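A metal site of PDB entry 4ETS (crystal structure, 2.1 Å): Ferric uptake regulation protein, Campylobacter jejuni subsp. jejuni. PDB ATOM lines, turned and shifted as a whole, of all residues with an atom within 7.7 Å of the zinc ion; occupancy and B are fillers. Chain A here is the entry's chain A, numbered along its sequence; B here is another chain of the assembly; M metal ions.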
ATOM      1  N   ILE A 109      -2.607  14.808 -16.281  1.00  0.00           N
ATOM      2  CA  ILE A 109      -1.503  14.359 -17.154  1.00  0.00           C
ATOM      3  C   ILE A 109      -1.722  12.908 -17.622  1.00  0.00           C
ATOM      4  O   ILE A 109      -1.914  12.046 -16.798  1.00  0.00           O
ATOM      5  CB  ILE A 109      -0.148  14.470 -16.368  1.00  0.00           C
ATOM      6  CG1 ILE A 109       0.087  15.930 -15.994  1.00  0.00           C
ATOM      7  CG2 ILE A 109       1.028  13.897 -17.170  1.00  0.00           C
ATOM      8  CD1 ILE A 109       1.129  16.195 -14.942  1.00  0.00           C
ATOM      9  N   CYS A 110      -1.683  12.648 -18.935  1.00  0.00           N
ATOM     10  CA  CYS A 110      -1.771  11.273 -19.426  1.00  0.00           C
ATOM     11  C   CYS A 110      -0.387  10.624 -19.211  1.00  0.00           C
ATOM     12  O   CYS A 110       0.559  11.136 -19.721  1.00  0.00           O
ATOM     13  CB  CYS A 110      -2.104  11.170 -20.936  1.00  0.00           C
ATOM     14  SG  CYS A 110      -2.055   9.430 -21.409  1.00  0.00           S
ATOM     15  N   LYS A 111      -0.347   9.505 -18.480  1.00  0.00           N
ATOM     16  CA  LYS A 111       0.910   8.764 -18.126  1.00  0.00           C
ATOM     17  C   LYS A 111       1.597   8.195 -19.415  1.00  0.00           C
ATOM     18  O   LYS A 111       2.799   7.951 -19.434  1.00  0.00           O
ATOM     19  CB  LYS A 111       0.600   7.600 -17.142  1.00  0.00           C
ATOM     20  CG  LYS A 111       0.409   8.065 -15.671  1.00  0.00           C
ATOM     21  CD  LYS A 111       0.209   6.922 -14.549  1.00  0.00           C
ATOM     22  CE  LYS A 111      -0.645   7.530 -13.326  1.00  0.00           C
ATOM     23  NZ  LYS A 111      -0.673   7.024 -11.802  1.00  0.00           N
ATOM     24  N   ASN A 112       0.835   8.029 -20.467  1.00  0.00           N
ATOM     25  CA  ASN A 112       1.405   7.499 -21.699  1.00  0.00           C
ATOM     26  C   ASN A 112       1.911   8.553 -22.679  1.00  0.00           C
ATOM     27  O   ASN A 112       3.122   8.774 -22.805  1.00  0.00           O
ATOM     28  CB  ASN A 112       0.439   6.541 -22.381  1.00  0.00           C
ATOM     29  CG  ASN A 112       1.106   5.753 -23.507  1.00  0.00           C
ATOM     30  OD1 ASN A 112       2.122   6.192 -24.086  1.00  0.00           O
ATOM     31  ND2 ASN A 112       0.520   4.593 -23.840  1.00  0.00           N
ATOM     32  N   CYS A 113       1.002   9.215 -23.372  1.00  0.00           N
ATOM     33  CA  CYS A 113       1.446  10.162 -24.399  1.00  0.00           C
ATOM     34  C   CYS A 113       1.904  11.491 -23.849  1.00  0.00           C
ATOM     35  O   CYS A 113       2.371  12.305 -24.608  1.00  0.00           O
ATOM     36  CB  CYS A 113       0.293  10.413 -25.375  1.00  0.00           C
ATOM     37  SG  CYS A 113      -1.241  11.168 -24.604  1.00  0.00           S
ATOM     38  N   GLY A 114       1.674  11.772 -22.553  1.00  0.00           N
ATOM     39  CA  GLY A 114       2.052  13.074 -21.987  1.00  0.00           C
ATOM     40  C   GLY A 114       1.136  14.240 -22.350  1.00  0.00           C
ATOM     41  O   GLY A 114       1.495  15.363 -22.178  1.00  0.00           O
ATOM     42  N   LYS A 115      -0.038  14.004 -22.875  1.00  0.00           N
ATOM     43  CA  LYS A 115      -1.034  15.077 -23.063  1.00  0.00           C
ATOM     44  C   LYS A 115      -1.435  15.682 -21.681  1.00  0.00           C
ATOM     45  O   LYS A 115      -1.584  14.946 -20.698  1.00  0.00           O
ATOM     46  CB  LYS A 115      -2.257  14.442 -23.713  1.00  0.00           C
ATOM     47  CG  LYS A 115      -3.525  15.211 -23.535  1.00  0.00           C
ATOM     48  CD  LYS A 115      -4.685  14.451 -24.110  1.00  0.00           C
ATOM     49  CE  LYS A 115      -5.833  15.402 -24.433  1.00  0.00           C
ATOM     50  NZ  LYS A 115      -7.119  14.634 -24.548  1.00  0.00           N
ATOM     51  N   ILE A 116      -1.655  17.006 -21.632  1.00  0.00           N
ATOM     52  CA  ILE A 116      -1.929  17.662 -20.390  1.00  0.00           C
ATOM     53  C   ILE A 116      -3.225  18.441 -20.574  1.00  0.00           C
ATOM     54  O   ILE A 116      -3.425  19.092 -21.592  1.00  0.00           O
ATOM     55  CB  ILE A 116      -0.863  18.637 -19.965  1.00  0.00           C
ATOM     56  CG1 ILE A 116       0.543  17.995 -19.935  1.00  0.00           C
ATOM     57  CG2 ILE A 116      -1.216  19.330 -18.625  1.00  0.00           C
ATOM     58  CD1 ILE A 116       0.563  16.638 -19.468  1.00  0.00           C
ATOM     59  N   GLY A 148      -3.413   9.936 -15.105  1.00  0.00           N
ATOM     60  CA  GLY A 148      -4.291   8.935 -15.678  1.00  0.00           C
ATOM     61  C   GLY A 148      -3.866   8.558 -17.079  1.00  0.00           C
ATOM     62  O   GLY A 148      -2.718   8.789 -17.465  1.00  0.00           O
ATOM     63  N   VAL A 149      -4.775   7.938 -17.831  1.00  0.00           N
ATOM     64  CA  VAL A 149      -4.453   7.550 -19.192  1.00  0.00           C
ATOM     65  C   VAL A 149      -5.583   8.109 -20.032  1.00  0.00           C
ATOM     66  O   VAL A 149      -6.754   7.908 -19.728  1.00  0.00           O
ATOM     67  CB  VAL A 149      -4.325   5.985 -19.364  1.00  0.00           C
ATOM     68  CG1 VAL A 149      -4.158   5.600 -20.816  1.00  0.00           C
ATOM     69  CG2 VAL A 149      -3.101   5.409 -18.533  1.00  0.00           C
ATOM     70  N   CYS A 150      -5.231   8.842 -21.076  1.00  0.00           N
ATOM     71  CA  CYS A 150      -6.282   9.443 -21.904  1.00  0.00           C
ATOM     72  C   CYS A 150      -7.029   8.380 -22.713  1.00  0.00           C
ATOM     73  O   CYS A 150      -6.650   7.177 -22.718  1.00  0.00           O
ATOM     74  CB  CYS A 150      -5.704  10.547 -22.813  1.00  0.00           C
ATOM     75  SG  CYS A 150      -4.765   9.891 -24.226  1.00  0.00           S
ATOM     76  N   GLY A 151      -8.114   8.842 -23.363  1.00  0.00           N
ATOM     77  CA  GLY A 151      -8.995   8.008 -24.182  1.00  0.00           C
ATOM     78  C   GLY A 151      -8.240   7.362 -25.329  1.00  0.00           C
ATOM     79  O   GLY A 151      -8.398   6.159 -25.593  1.00  0.00           O
ATOM     80  N   ASP A 152      -7.394   8.129 -25.978  1.00  0.00           N
ATOM     81  CA  ASP A 152      -6.566   7.583 -27.052  1.00  0.00           C
ATOM     82  C   ASP A 152      -5.557   6.527 -26.566  1.00  0.00           C
ATOM     83  O   ASP A 152      -5.315   5.552 -27.278  1.00  0.00           O
ATOM     84  CB  ASP A 152      -5.827   8.705 -27.777  1.00  0.00           C
ATOM     85  CG  ASP A 152      -6.774   9.705 -28.403  1.00  0.00           C
ATOM     86  OD1 ASP A 152      -7.946   9.364 -28.633  1.00  0.00           O
ATOM     87  OD2 ASP A 152      -6.333  10.840 -28.693  1.00  0.00           O
ATOM     88  N   CYS A 153      -4.954   6.713 -25.400  1.00  0.00           N
ATOM     89  CA  CYS A 153      -3.988   5.721 -24.914  1.00  0.00           C
ATOM     90  C   CYS A 153      -4.628   4.628 -24.077  1.00  0.00           C
ATOM     91  O   CYS A 153      -3.902   3.835 -23.465  1.00  0.00           O
ATOM     92  CB  CYS A 153      -2.883   6.377 -24.077  1.00  0.00           C
ATOM     93  SG  CYS A 153      -1.942   7.589 -24.917  1.00  0.00           S
ATOM     94  N   ASN A 154      -5.958   4.654 -23.951  1.00  0.00           N
ATOM     95  CA  ASN A 154      -6.752   3.660 -23.226  1.00  0.00           C
ATOM     96  C   ASN A 154      -7.868   4.073 -22.279  1.00  0.00           C
ATOM     97  O   ASN A 154      -8.317   3.238 -21.477  1.00  0.00           O
ATOM     98  CB  ASN A 154      -5.863   2.595 -22.561  1.00  0.00           C
ATOM     99  CG  ASN A 154      -5.707   1.385 -23.431  1.00  0.00           C
ATOM    100  OD1 ASN A 154      -5.532   1.544 -24.648  1.00  0.00           O
ATOM    101  ND2 ASN A 154      -5.825   0.159 -22.851  1.00  0.00           N
ATOM    102  N   PHE B 137     -10.556  10.520 -19.692  1.00  0.00           N
ATOM    103  CA  PHE B 137      -9.400   9.889 -19.003  1.00  0.00           C
ATOM    104  C   PHE B 137      -9.869   8.901 -18.010  1.00  0.00           C
ATOM    105  O   PHE B 137     -10.970   9.043 -17.426  1.00  0.00           O
ATOM    106  CB  PHE B 137      -8.573  10.876 -18.157  1.00  0.00           C
ATOM    107  CG  PHE B 137      -7.516  11.655 -18.899  1.00  0.00           C
ATOM    108  CD1 PHE B 137      -7.860  12.486 -19.979  1.00  0.00           C
ATOM    109  CD2 PHE B 137      -6.199  11.587 -18.499  1.00  0.00           C
ATOM    110  CE1 PHE B 137      -6.885  13.208 -20.658  1.00  0.00           C
ATOM    111  CE2 PHE B 137      -5.198  12.319 -19.141  1.00  0.00           C
ATOM    112  CZ  PHE B 137      -5.519  13.133 -20.246  1.00  0.00           C
HETATM  113 ZN    ZN M   1      -2.550   9.707 -23.743  1.00  0.00          ZN
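SG of Cys 110 lies close to N of Asn 112 (3.3 Å). The backbone NH (N) of Cys 110 lies within hydrogen-bond range of the backbone carbonyl oxygen (O) of Lys 115 (2.9 Å). The side-chain sulfur of Cys 150 sits close to the backbone NH of Asp 152. The side-chain sulfur (SG) of Cys 113 sits close to the backbone NH (N) of Lys 115, at 3.5 Å.
Of the 16 residues printed, 4 come within 4 Å of the zinc ion.
The side-chain sulfur (SG) of Cys 113 is bound to the zinc ion, at 2.1 Å. SG of Cys 150 binds the zinc ion (2.3 Å). SG of Cys 110 is bound to the zinc ion (2.4 Å). The zinc ion is bound by SG of Cys 153.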
